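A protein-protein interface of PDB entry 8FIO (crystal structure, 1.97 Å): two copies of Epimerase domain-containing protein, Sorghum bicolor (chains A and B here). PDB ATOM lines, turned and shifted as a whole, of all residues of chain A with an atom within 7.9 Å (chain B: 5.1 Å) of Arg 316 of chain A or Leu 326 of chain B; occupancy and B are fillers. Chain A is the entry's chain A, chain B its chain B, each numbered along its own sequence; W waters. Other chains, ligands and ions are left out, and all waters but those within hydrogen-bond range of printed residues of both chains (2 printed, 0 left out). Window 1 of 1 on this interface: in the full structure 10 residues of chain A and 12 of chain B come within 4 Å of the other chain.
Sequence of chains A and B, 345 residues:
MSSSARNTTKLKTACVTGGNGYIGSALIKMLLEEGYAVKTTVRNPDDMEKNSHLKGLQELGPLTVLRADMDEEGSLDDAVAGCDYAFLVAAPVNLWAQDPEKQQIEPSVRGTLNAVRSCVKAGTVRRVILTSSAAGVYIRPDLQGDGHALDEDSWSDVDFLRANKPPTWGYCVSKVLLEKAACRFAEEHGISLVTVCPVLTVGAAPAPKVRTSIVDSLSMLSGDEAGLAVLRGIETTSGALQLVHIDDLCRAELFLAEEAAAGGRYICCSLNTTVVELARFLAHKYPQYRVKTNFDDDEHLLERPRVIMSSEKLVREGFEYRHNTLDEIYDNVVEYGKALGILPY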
ATOM      1  N   PHE A 255      -0.536  16.739  38.895  1.00  0.00           N
ATOM      2  CA  PHE A 255       0.411  17.764  38.469  1.00  0.00           C
ATOM      3  C   PHE A 255      -0.138  19.165  38.718  1.00  0.00           C
ATOM      4  O   PHE A 255       0.541  20.022  39.294  1.00  0.00           O
ATOM      5  CB  PHE A 255       0.751  17.582  36.989  1.00  0.00           C
ATOM      6  CG  PHE A 255       1.550  18.715  36.420  1.00  0.00           C
ATOM      7  CD1 PHE A 255       2.920  18.783  36.619  1.00  0.00           C
ATOM      8  CD2 PHE A 255       0.925  19.733  35.707  1.00  0.00           C
ATOM      9  CE1 PHE A 255       3.657  19.834  36.103  1.00  0.00           C
ATOM     10  CE2 PHE A 255       1.659  20.785  35.190  1.00  0.00           C
ATOM     11  CZ  PHE A 255       3.026  20.831  35.389  1.00  0.00           C
ATOM     12  N   GLU A 259       1.576  21.951  41.127  1.00  0.00           N
ATOM     13  CA  GLU A 259       2.359  22.950  40.397  1.00  0.00           C
ATOM     14  C   GLU A 259       1.871  24.335  40.808  1.00  0.00           C
ATOM     15  O   GLU A 259       0.813  24.792  40.364  1.00  0.00           O
ATOM     16  CB  GLU A 259       2.239  22.732  38.894  1.00  0.00           C
ATOM     17  CG  GLU A 259       3.002  23.730  38.044  1.00  0.00           C
ATOM     18  CD  GLU A 259       4.448  23.892  38.487  1.00  0.00           C
ATOM     19  OE1 GLU A 259       5.292  23.066  38.082  1.00  0.00           O
ATOM     20  OE2 GLU A 259       4.742  24.854  39.238  1.00  0.00           O
ATOM     21  N   TYR A 266      -7.645  24.267  32.160  1.00  0.00           N
ATOM     22  CA  TYR A 266      -6.715  23.432  31.404  1.00  0.00           C
ATOM     23  C   TYR A 266      -7.475  22.381  30.613  1.00  0.00           C
ATOM     24  O   TYR A 266      -8.237  21.600  31.189  1.00  0.00           O
ATOM     25  CB  TYR A 266      -5.700  22.746  32.324  1.00  0.00           C
ATOM     26  CG  TYR A 266      -4.659  23.670  32.902  1.00  0.00           C
ATOM     27  CD1 TYR A 266      -4.922  24.413  34.044  1.00  0.00           C
ATOM     28  CD2 TYR A 266      -3.408  23.795  32.309  1.00  0.00           C
ATOM     29  CE1 TYR A 266      -3.973  25.265  34.577  1.00  0.00           C
ATOM     30  CE2 TYR A 266      -2.447  24.648  32.840  1.00  0.00           C
ATOM     31  CZ  TYR A 266      -2.740  25.381  33.972  1.00  0.00           C
ATOM     32  OH  TYR A 266      -1.796  26.226  34.507  1.00  0.00           O
ATOM     33  N   SER A 310      -6.320  21.699  21.518  1.00  0.00           N
ATOM     34  CA  SER A 310      -4.906  21.919  21.790  1.00  0.00           C
ATOM     35  C   SER A 310      -4.653  21.802  23.287  1.00  0.00           C
ATOM     36  O   SER A 310      -5.280  22.510  24.084  1.00  0.00           O
ATOM     37  CB  SER A 310      -4.458  23.289  21.286  1.00  0.00           C
ATOM     38  OG  SER A 310      -3.100  23.523  21.630  1.00  0.00           O
ATOM     39  N   SER A 311      -3.729  20.916  23.665  1.00  0.00           N
ATOM     40  CA  SER A 311      -3.267  20.797  25.040  1.00  0.00           C
ATOM     41  C   SER A 311      -1.975  21.572  25.277  1.00  0.00           C
ATOM     42  O   SER A 311      -1.188  21.212  26.158  1.00  0.00           O
ATOM     43  CB  SER A 311      -3.083  19.326  25.412  1.00  0.00           C
ATOM     44  OG  SER A 311      -2.728  19.185  26.775  1.00  0.00           O
ATOM     45  N   GLU A 312      -1.745  22.643  24.514  1.00  0.00           N
ATOM     46  CA  GLU A 312      -0.466  23.338  24.608  1.00  0.00           C
ATOM     47  C   GLU A 312      -0.285  23.989  25.978  1.00  0.00           C
ATOM     48  O   GLU A 312       0.829  24.014  26.514  1.00  0.00           O
ATOM     49  CB  GLU A 312      -0.341  24.376  23.493  1.00  0.00           C
ATOM     50  CG  GLU A 312       0.524  25.575  23.859  1.00  0.00           C
ATOM     51  CD  GLU A 312       0.762  26.513  22.689  1.00  0.00           C
ATOM     52  OE1 GLU A 312       0.403  26.160  21.544  1.00  0.00           O
ATOM     53  OE2 GLU A 312       1.322  27.606  22.913  1.00  0.00           O
ATOM     54  N   LYS A 313      -1.363  24.511  26.566  1.00  0.00           N
ATOM     55  CA  LYS A 313      -1.227  25.177  27.859  1.00  0.00           C
ATOM     56  C   LYS A 313      -0.775  24.196  28.936  1.00  0.00           C
ATOM     57  O   LYS A 313       0.132  24.490  29.724  1.00  0.00           O
ATOM     58  CB  LYS A 313      -2.541  25.849  28.257  1.00  0.00           C
ATOM     59  CG  LYS A 313      -2.434  26.648  29.553  1.00  0.00           C
ATOM     60  CD  LYS A 313      -3.776  27.205  30.000  1.00  0.00           C
ATOM     61  CE  LYS A 313      -3.682  27.835  31.384  1.00  0.00           C
ATOM     62  NZ  LYS A 313      -5.003  28.342  31.863  1.00  0.00           N
ATOM     63  N   LEU A 314      -1.397  23.017  28.984  1.00  0.00           N
ATOM     64  CA  LEU A 314      -1.013  22.024  29.981  1.00  0.00           C
ATOM     65  C   LEU A 314       0.404  21.513  29.740  1.00  0.00           C
ATOM     66  O   LEU A 314       1.178  21.330  30.688  1.00  0.00           O
ATOM     67  CB  LEU A 314      -2.015  20.870  29.977  1.00  0.00           C
ATOM     68  CG  LEU A 314      -1.770  19.709  30.943  1.00  0.00           C
ATOM     69  CD1 LEU A 314      -1.669  20.201  32.382  1.00  0.00           C
ATOM     70  CD2 LEU A 314      -2.873  18.657  30.803  1.00  0.00           C
ATOM     71  N   VAL A 315       0.768  21.281  28.477  1.00  0.00           N
ATOM     72  CA  VAL A 315       2.106  20.782  28.179  1.00  0.00           C
ATOM     73  C   VAL A 315       3.153  21.845  28.491  1.00  0.00           C
ATOM     74  O   VAL A 315       4.218  21.546  29.045  1.00  0.00           O
ATOM     75  CB  VAL A 315       2.189  20.317  26.715  1.00  0.00           C
ATOM     76  CG1 VAL A 315       3.642  20.151  26.296  1.00  0.00           C
ATOM     77  CG2 VAL A 315       1.415  19.016  26.524  1.00  0.00           C
ATOM     78  N   ARG A 316       2.874  23.102  28.139  1.00  0.00           N
ATOM     79  CA  ARG A 316       3.795  24.179  28.485  1.00  0.00           C
ATOM     80  C   ARG A 316       3.953  24.298  29.994  1.00  0.00           C
ATOM     81  O   ARG A 316       5.057  24.549  30.496  1.00  0.00           O
ATOM     82  CB  ARG A 316       3.307  25.500  27.892  1.00  0.00           C
ATOM     83  CG  ARG A 316       3.535  25.631  26.388  1.00  0.00           C
ATOM     84  CD  ARG A 316       3.078  27.004  25.898  1.00  0.00           C
ATOM     85  NE  ARG A 316       3.806  28.080  26.561  1.00  0.00           N
ATOM     86  CZ  ARG A 316       3.754  29.354  26.202  1.00  0.00           C
ATOM     87  NH1 ARG A 316       2.978  29.760  25.210  1.00  0.00           N
ATOM     88  NH2 ARG A 316       4.489  30.246  26.863  1.00  0.00           N
ATOM     89  N   GLU A 317       2.857  24.117  30.736  1.00  0.00           N
ATOM     90  CA  GLU A 317       2.927  24.200  32.190  1.00  0.00           C
ATOM     91  C   GLU A 317       3.929  23.206  32.763  1.00  0.00           C
ATOM     92  O   GLU A 317       4.537  23.470  33.805  1.00  0.00           O
ATOM     93  CB  GLU A 317       1.542  23.971  32.796  1.00  0.00           C
ATOM     94  CG  GLU A 317       1.397  24.506  34.211  1.00  0.00           C
ATOM     95  CD  GLU A 317       1.408  26.017  34.250  1.00  0.00           C
ATOM     96  OE1 GLU A 317       0.509  26.633  33.638  1.00  0.00           O
ATOM     97  OE2 GLU A 317       2.323  26.587  34.885  1.00  0.00           O
ATOM     98  N   GLY A 318       4.117  22.065  32.104  1.00  0.00           N
ATOM     99  CA  GLY A 318       5.111  21.107  32.549  1.00  0.00           C
ATOM    100  C   GLY A 318       4.684  19.658  32.458  1.00  0.00           C
ATOM    101  O   GLY A 318       5.482  18.764  32.750  1.00  0.00           O
ATOM    102  N   PHE A 319       3.437  19.406  32.061  1.00  0.00           N
ATOM    103  CA  PHE A 319       2.911  18.051  31.990  1.00  0.00           C
ATOM    104  C   PHE A 319       3.263  17.399  30.657  1.00  0.00           C
ATOM    105  O   PHE A 319       3.299  18.052  29.608  1.00  0.00           O
ATOM    106  CB  PHE A 319       1.391  18.042  32.178  1.00  0.00           C
ATOM    107  CG  PHE A 319       0.772  16.673  32.063  1.00  0.00           C
ATOM    108  CD1 PHE A 319       0.820  15.782  33.125  1.00  0.00           C
ATOM    109  CD2 PHE A 319       0.144  16.276  30.891  1.00  0.00           C
ATOM    110  CE1 PHE A 319       0.257  14.517  33.020  1.00  0.00           C
ATOM    111  CE2 PHE A 319      -0.427  15.015  30.779  1.00  0.00           C
ATOM    112  CZ  PHE A 319      -0.372  14.135  31.852  1.00  0.00           C
ATOM    113  N   GLU A 320       3.505  16.094  30.707  1.00  0.00           N
ATOM    114  CA  GLU A 320       3.791  15.303  29.517  1.00  0.00           C
ATOM    115  C   GLU A 320       2.886  14.081  29.483  1.00  0.00           C
ATOM    116  O   GLU A 320       2.810  13.336  30.465  1.00  0.00           O
ATOM    117  CB  GLU A 320       5.264  14.873  29.471  1.00  0.00           C
ATOM    118  CG  GLU A 320       6.228  16.044  29.303  1.00  0.00           C
ATOM    119  CD  GLU A 320       7.653  15.677  29.662  1.00  0.00           C
ATOM    120  OE1 GLU A 320       7.946  15.480  30.862  1.00  0.00           O
ATOM    121  OE2 GLU A 320       8.479  15.576  28.736  1.00  0.00           O
ATOM    122  N   LEU B 243       9.563  34.394  20.424  1.00  0.00           N
ATOM    123  CA  LEU B 243       9.207  33.888  19.106  1.00  0.00           C
ATOM    124  C   LEU B 243       8.210  34.801  18.409  1.00  0.00           C
ATOM    125  O   LEU B 243       7.420  35.504  19.048  1.00  0.00           O
ATOM    126  CB  LEU B 243       8.606  32.481  19.175  1.00  0.00           C
ATOM    127  CG  LEU B 243       9.447  31.378  19.808  1.00  0.00           C
ATOM    128  CD1 LEU B 243       8.604  30.140  20.041  1.00  0.00           C
ATOM    129  CD2 LEU B 243      10.649  31.068  18.916  1.00  0.00           C
ATOM    130  N   LEU B 271       5.347  36.037  21.470  1.00  0.00           N
ATOM    131  CA  LEU B 271       5.238  35.126  22.599  1.00  0.00           C
ATOM    132  C   LEU B 271       6.594  34.977  23.271  1.00  0.00           C
ATOM    133  O   LEU B 271       7.628  34.941  22.596  1.00  0.00           O
ATOM    134  CB  LEU B 271       4.705  33.770  22.116  1.00  0.00           C
ATOM    135  CG  LEU B 271       4.718  32.497  22.952  1.00  0.00           C
ATOM    136  CD1 LEU B 271       3.715  31.523  22.348  1.00  0.00           C
ATOM    137  CD2 LEU B 271       6.105  31.875  22.995  1.00  0.00           C
ATOM    138  N   ASN B 272       6.579  34.908  24.600  1.00  0.00           N
ATOM    139  CA  ASN B 272       7.770  34.656  25.400  1.00  0.00           C
ATOM    140  C   ASN B 272       7.649  33.270  26.022  1.00  0.00           C
ATOM    141  O   ASN B 272       6.721  33.013  26.797  1.00  0.00           O
ATOM    142  CB  ASN B 272       7.941  35.715  26.488  1.00  0.00           C
ATOM    143  CG  ASN B 272       8.214  37.094  25.924  1.00  0.00           C
ATOM    144  OD1 ASN B 272       9.367  37.478  25.727  1.00  0.00           O
ATOM    145  ND2 ASN B 272       7.152  37.853  25.668  1.00  0.00           N
ATOM    146  N   THR B 273       8.578  32.385  25.683  1.00  0.00           N
ATOM    147  CA  THR B 273       8.580  31.032  26.224  1.00  0.00           C
ATOM    148  C   THR B 273       9.992  30.715  26.715  1.00  0.00           C
ATOM    149  O   THR B 273      10.826  31.604  26.924  1.00  0.00           O
ATOM    150  CB  THR B 273       8.077  30.026  25.179  1.00  0.00           C
ATOM    151  OG1 THR B 273       8.018  28.715  25.758  1.00  0.00           O
ATOM    152  CG2 THR B 273       8.999  30.005  23.963  1.00  0.00           C
ATOM    153  N   GLU B 277       9.888  24.759  27.785  1.00  0.00           N
ATOM    154  CA  GLU B 277       8.499  24.818  27.341  1.00  0.00           C
ATOM    155  C   GLU B 277       8.382  24.417  25.878  1.00  0.00           C
ATOM    156  O   GLU B 277       7.535  23.594  25.509  1.00  0.00           O
ATOM    157  CB  GLU B 277       7.949  26.229  27.548  1.00  0.00           C
ATOM    158  CG  GLU B 277       7.173  26.439  28.820  1.00  0.00           C
ATOM    159  CD  GLU B 277       6.830  27.900  29.037  1.00  0.00           C
ATOM    160  OE1 GLU B 277       6.296  28.529  28.100  1.00  0.00           O
ATOM    161  OE2 GLU B 277       7.090  28.418  30.146  1.00  0.00           O
ATOM    162  N   LEU B 278       9.226  24.998  25.023  1.00  0.00           N
ATOM    163  CA  LEU B 278       9.167  24.690  23.598  1.00  0.00           C
ATOM    164  C   LEU B 278       9.495  23.225  23.340  1.00  0.00           C
ATOM    165  O   LEU B 278       8.849  22.570  22.512  1.00  0.00           O
ATOM    166  CB  LEU B 278      10.127  25.600  22.832  1.00  0.00           C
ATOM    167  CG  LEU B 278      10.194  25.433  21.317  1.00  0.00           C
ATOM    168  CD1 LEU B 278       8.834  25.706  20.688  1.00  0.00           C
ATOM    169  CD2 LEU B 278      11.267  26.356  20.731  1.00  0.00           C
ATOM    170  N   ARG B 280       9.008  20.630  25.329  1.00  0.00           N
ATOM    171  CA  ARG B 280       7.851  19.814  25.687  1.00  0.00           C
ATOM    172  C   ARG B 280       6.760  19.915  24.631  1.00  0.00           C
ATOM    173  O   ARG B 280       6.191  18.901  24.210  1.00  0.00           O
ATOM    174  CB  ARG B 280       7.295  20.227  27.048  1.00  0.00           C
ATOM    175  CG  ARG B 280       8.176  19.949  28.244  1.00  0.00           C
ATOM    176  CD  ARG B 280       7.291  19.999  29.488  1.00  0.00           C
ATOM    177  NE  ARG B 280       7.223  21.343  30.043  1.00  0.00           N
ATOM    178  CZ  ARG B 280       8.120  21.863  30.865  1.00  0.00           C
ATOM    179  NH1 ARG B 280       9.110  21.135  31.352  1.00  0.00           N
ATOM    180  NH2 ARG B 280       8.000  23.136  31.231  1.00  0.00           N
ATOM    181  N   PHE B 281       6.433  21.140  24.211  1.00  0.00           N
ATOM    182  CA  PHE B 281       5.353  21.314  23.246  1.00  0.00           C
ATOM    183  C   PHE B 281       5.679  20.629  21.925  1.00  0.00           C
ATOM    184  O   PHE B 281       4.832  19.942  21.339  1.00  0.00           O
ATOM    185  CB  PHE B 281       5.063  22.795  23.004  1.00  0.00           C
ATOM    186  CG  PHE B 281       4.038  23.018  21.933  1.00  0.00           C
ATOM    187  CD1 PHE B 281       2.692  22.816  22.196  1.00  0.00           C
ATOM    188  CD2 PHE B 281       4.422  23.365  20.649  1.00  0.00           C
ATOM    189  CE1 PHE B 281       1.743  22.991  21.203  1.00  0.00           C
ATOM    190  CE2 PHE B 281       3.480  23.537  19.654  1.00  0.00           C
ATOM    191  CZ  PHE B 281       2.138  23.346  19.932  1.00  0.00           C
ATOM    192  N   ASN B 324      -0.524  33.356  17.789  1.00  0.00           N
ATOM    193  CA  ASN B 324      -0.446  33.754  19.187  1.00  0.00           C
ATOM    194  C   ASN B 324      -0.113  32.608  20.132  1.00  0.00           C
ATOM    195  O   ASN B 324       0.037  32.842  21.338  1.00  0.00           O
ATOM    196  CB  ASN B 324      -1.766  34.413  19.599  1.00  0.00           C
ATOM    197  CG  ASN B 324      -2.060  35.656  18.786  1.00  0.00           C
ATOM    198  OD1 ASN B 324      -1.357  36.657  18.898  1.00  0.00           O
ATOM    199  ND2 ASN B 324      -3.079  35.587  17.933  1.00  0.00           N
ATOM    200  N   THR B 325       0.012  31.388  19.625  1.00  0.00           N
ATOM    201  CA  THR B 325       0.371  30.238  20.437  1.00  0.00           C
ATOM    202  C   THR B 325       1.550  29.524  19.792  1.00  0.00           C
ATOM    203  O   THR B 325       1.867  29.744  18.620  1.00  0.00           O
ATOM    204  CB  THR B 325      -0.803  29.262  20.593  1.00  0.00           C
ATOM    205  OG1 THR B 325      -1.064  28.634  19.331  1.00  0.00           O
ATOM    206  CG2 THR B 325      -2.051  29.997  21.051  1.00  0.00           C
ATOM    207  N   LEU B 326       2.199  28.656  20.572  1.00  0.00           N
ATOM    208  CA  LEU B 326       3.262  27.835  20.001  1.00  0.00           C
ATOM    209  C   LEU B 326       2.735  26.985  18.855  1.00  0.00           C
ATOM    210  O   LEU B 326       3.453  26.737  17.877  1.00  0.00           O
ATOM    211  CB  LEU B 326       3.888  26.948  21.080  1.00  0.00           C
ATOM    212  CG  LEU B 326       4.692  27.642  22.179  1.00  0.00           C
ATOM    213  CD1 LEU B 326       5.296  26.603  23.131  1.00  0.00           C
ATOM    214  CD2 LEU B 326       5.776  28.543  21.589  1.00  0.00           C
ATOM    215  N   ASP B 327       1.482  26.535  18.954  1.00  0.00           N
ATOM    216  CA  ASP B 327       0.896  25.734  17.887  1.00  0.00           C
ATOM    217  C   ASP B 327       0.769  26.537  16.601  1.00  0.00           C
ATOM    218  O   ASP B 327       0.942  25.992  15.504  1.00  0.00           O
ATOM    219  CB  ASP B 327      -0.470  25.202  18.318  1.00  0.00           C
ATOM    220  CG  ASP B 327      -0.992  24.125  17.393  1.00  0.00           C
ATOM    221  OD1 ASP B 327      -0.249  23.166  17.111  1.00  0.00           O
ATOM    222  OD2 ASP B 327      -2.140  24.259  16.923  1.00  0.00           O
ATOM    223  N   GLU B 328       0.465  27.835  16.712  1.00  0.00           N
ATOM    224  CA  GLU B 328       0.284  28.664  15.527  1.00  0.00           C
ATOM    225  C   GLU B 328       1.610  29.217  15.010  1.00  0.00           C
ATOM    226  O   GLU B 328       1.754  29.473  13.808  1.00  0.00           O
ATOM    227  CB  GLU B 328      -0.700  29.799  15.835  1.00  0.00           C
ATOM    228  CG  GLU B 328      -2.146  29.345  15.882  1.00  0.00           C
ATOM    229  CD  GLU B 328      -3.066  30.371  16.524  1.00  0.00           C
ATOM    230  OE1 GLU B 328      -2.561  31.359  17.097  1.00  0.00           O
ATOM    231  OE2 GLU B 328      -4.299  30.195  16.440  1.00  0.00           O
ATOM    232  N   ILE B 329       2.583  29.427  15.895  1.00  0.00           N
ATOM    233  CA  ILE B 329       3.886  29.895  15.440  1.00  0.00           C
ATOM    234  C   ILE B 329       4.609  28.789  14.682  1.00  0.00           C
ATOM    235  O   ILE B 329       5.308  29.045  13.695  1.00  0.00           O
ATOM    236  CB  ILE B 329       4.710  30.413  16.632  1.00  0.00           C
ATOM    237  CG1 ILE B 329       4.116  31.723  17.155  1.00  0.00           C
ATOM    238  CG2 ILE B 329       6.184  30.591  16.227  1.00  0.00           C
ATOM    239  CD1 ILE B 329       4.702  32.181  18.471  1.00  0.00           C
ATOM    240  N   TYR B 330       4.436  27.542  15.116  1.00  0.00           N
ATOM    241  CA  TYR B 330       5.026  26.381  14.455  1.00  0.00           C
ATOM    242  C   TYR B 330       4.026  25.676  13.554  1.00  0.00           C
ATOM    243  O   TYR B 330       3.943  24.446  13.561  1.00  0.00           O
ATOM    244  CB  TYR B 330       5.585  25.409  15.489  1.00  0.00           C
ATOM    245  CG  TYR B 330       6.988  25.738  15.941  1.00  0.00           C
ATOM    246  CD1 TYR B 330       7.222  26.716  16.903  1.00  0.00           C
ATOM    247  CD2 TYR B 330       8.082  25.073  15.401  1.00  0.00           C
ATOM    248  CE1 TYR B 330       8.513  27.012  17.320  1.00  0.00           C
ATOM    249  CE2 TYR B 330       9.372  25.364  15.808  1.00  0.00           C
ATOM    250  CZ  TYR B 330       9.583  26.331  16.763  1.00  0.00           C
ATOM    251  OH  TYR B 330      10.874  26.610  17.164  1.00  0.00           O
HETATM  252  O   HOH W   1       4.980  32.642  29.142  1.00  0.00           O
HETATM  253  O   HOH W   2       6.274  26.311  32.306  1.00  0.00           O
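No position is printed for both chains.
Of the 13 pairs that touch across the chains among the printed residues, none has its exchanged pair printed and touching as well.
Of chain B, only Leu 271 (3.4 Å), Asn 272 (3.6 Å), Thr 273 (3.97 Å), Glu 277 (2.8 Å), Arg 280 (3.3 Å) and Leu 326 (3.6 Å) come within 4 Å of Arg 316 of chain A.
Of the printed residues of chain A, Leu 326 of chain B touches Glu 312 and Arg 316.
Of the printed residues of chain A, Glu 277 of chain B touches Arg 316 (2.8 Å).
Printed residues of chain A within 4 Å of Asn 272 of chain B: Arg 316 (3.6 Å).
Printed residues of chain A within 4 Å of Leu 271 of chain B: Arg 316.
Printed residues of chain A within 4 Å of Phe 281 of chain B: Glu 312 (3.4 Å) and Val 315 (3.6 Å).
Phe 319 of chain A touches none of the printed residues of chain B.
The nearest residue of chain A that does not touch Leu 326 of chain B is Ser 310 of chain A (7.3 Å).
The nearest printed residue of chain A that does not touch Thr 273 of chain B is Glu 312 of chain A (7.4 Å).
The side-chain hydroxyl of Ser 310 of chain A sits close to the backbone NH of Glu 312 of chain A.
The guanidinium group (NH1) of Arg 316 of chain A is in salt-bridge range of the side-chain carboxylate (OE2) of Glu 312 of chain A, at 3.6 Å.
The backbone carbonyl oxygen (O) of Leu 271 of chain B is in hydrogen-bond range of the backbone NH (N) of Leu 243 of chain B.
The side-chain hydroxyl (OG1) of Thr 273 of chain B is in hydrogen-bond range of the side-chain carboxylate (OE1) of Glu 277 of chain B, 2.9 Å away.
OG1 of Thr 325 of chain B lies close to N of Asp 327 of chain B (3.3 Å).
The side-chain hydroxyl (OG1) of Thr 325 of chain B is in hydrogen-bond range of the backbone NH (N) of Glu 328 of chain B, at 3.1 Å.
Of the 15 printed residues of chain B, 9 touch a printed residue of chain A.
Of the 14 printed residues of chain A, 4 touch a printed residue of chain B.
Printed residues of chain A that touch a printed residue of chain B: Glu 312, Val 315, Arg 316 and Gly 318.
Among the printed residues, 13 pairs touch across the chains.
Among the printed residues, Asp or Glu carboxylates within 4 Å of a Lys or Arg side-chain nitrogen of the other chain: Arg 316 of chain A with Glu 277 of chain B (2.8 Å).
Among the printed residues, pairs that only touch across the chains: Gly 318 of chain A with Arg 280 of chain B (3.3 Å), Glu 312 of chain A with Phe 281 of chain B (3.4 Å), Arg 316 of chain A with Leu 271 of chain B (3.4 Å), Glu 312 of chain A with Thr 325 of chain B (3.5 Å), Arg 316 of chain A with Asn 272 of chain B (3.6 Å), Arg 316 of chain A with Leu 326 of chain B (3.6 Å), Val 315 of chain A with Phe 281 of chain B (3.6 Å) and Arg 316 of chain A with Thr 273 of chain B (3.97 Å).
OE2 of Glu 312 of chain A lies within hydrogen-bond range of N of Leu 326 of chain B, 2.7 Å away.
N of Asp 327 of chain B sits at hydrogen-bond distance from OE1 of Glu 312 of chain A (2.8 Å).
O of Val 315 of chain A sits at hydrogen-bond distance from NE of Arg 280 of chain B (3.2 Å).
The guanidinium group of Arg 316 of chain A is in salt-bridge range of the side-chain carboxylate of Glu 277 of chain B, at 2.8 Å.
The backbone carbonyl oxygen (O) of Arg 316 of chain A is in hydrogen-bond range of the guanidinium group (NH2) of Arg 280 of chain B (3.3 Å).
Water W2 lies within hydrogen-bond range of O of Arg 316 of chain A (2.8 Å) and OE2 of Glu 277 of chain B (3.1 Å).
Water W1 lies within hydrogen-bond range of the backbone carbonyl oxygen (O) of Asn 272 of chain B (2.9 Å) and the guanidinium group (NH2) of Arg 316 of chain A (3.3 Å).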
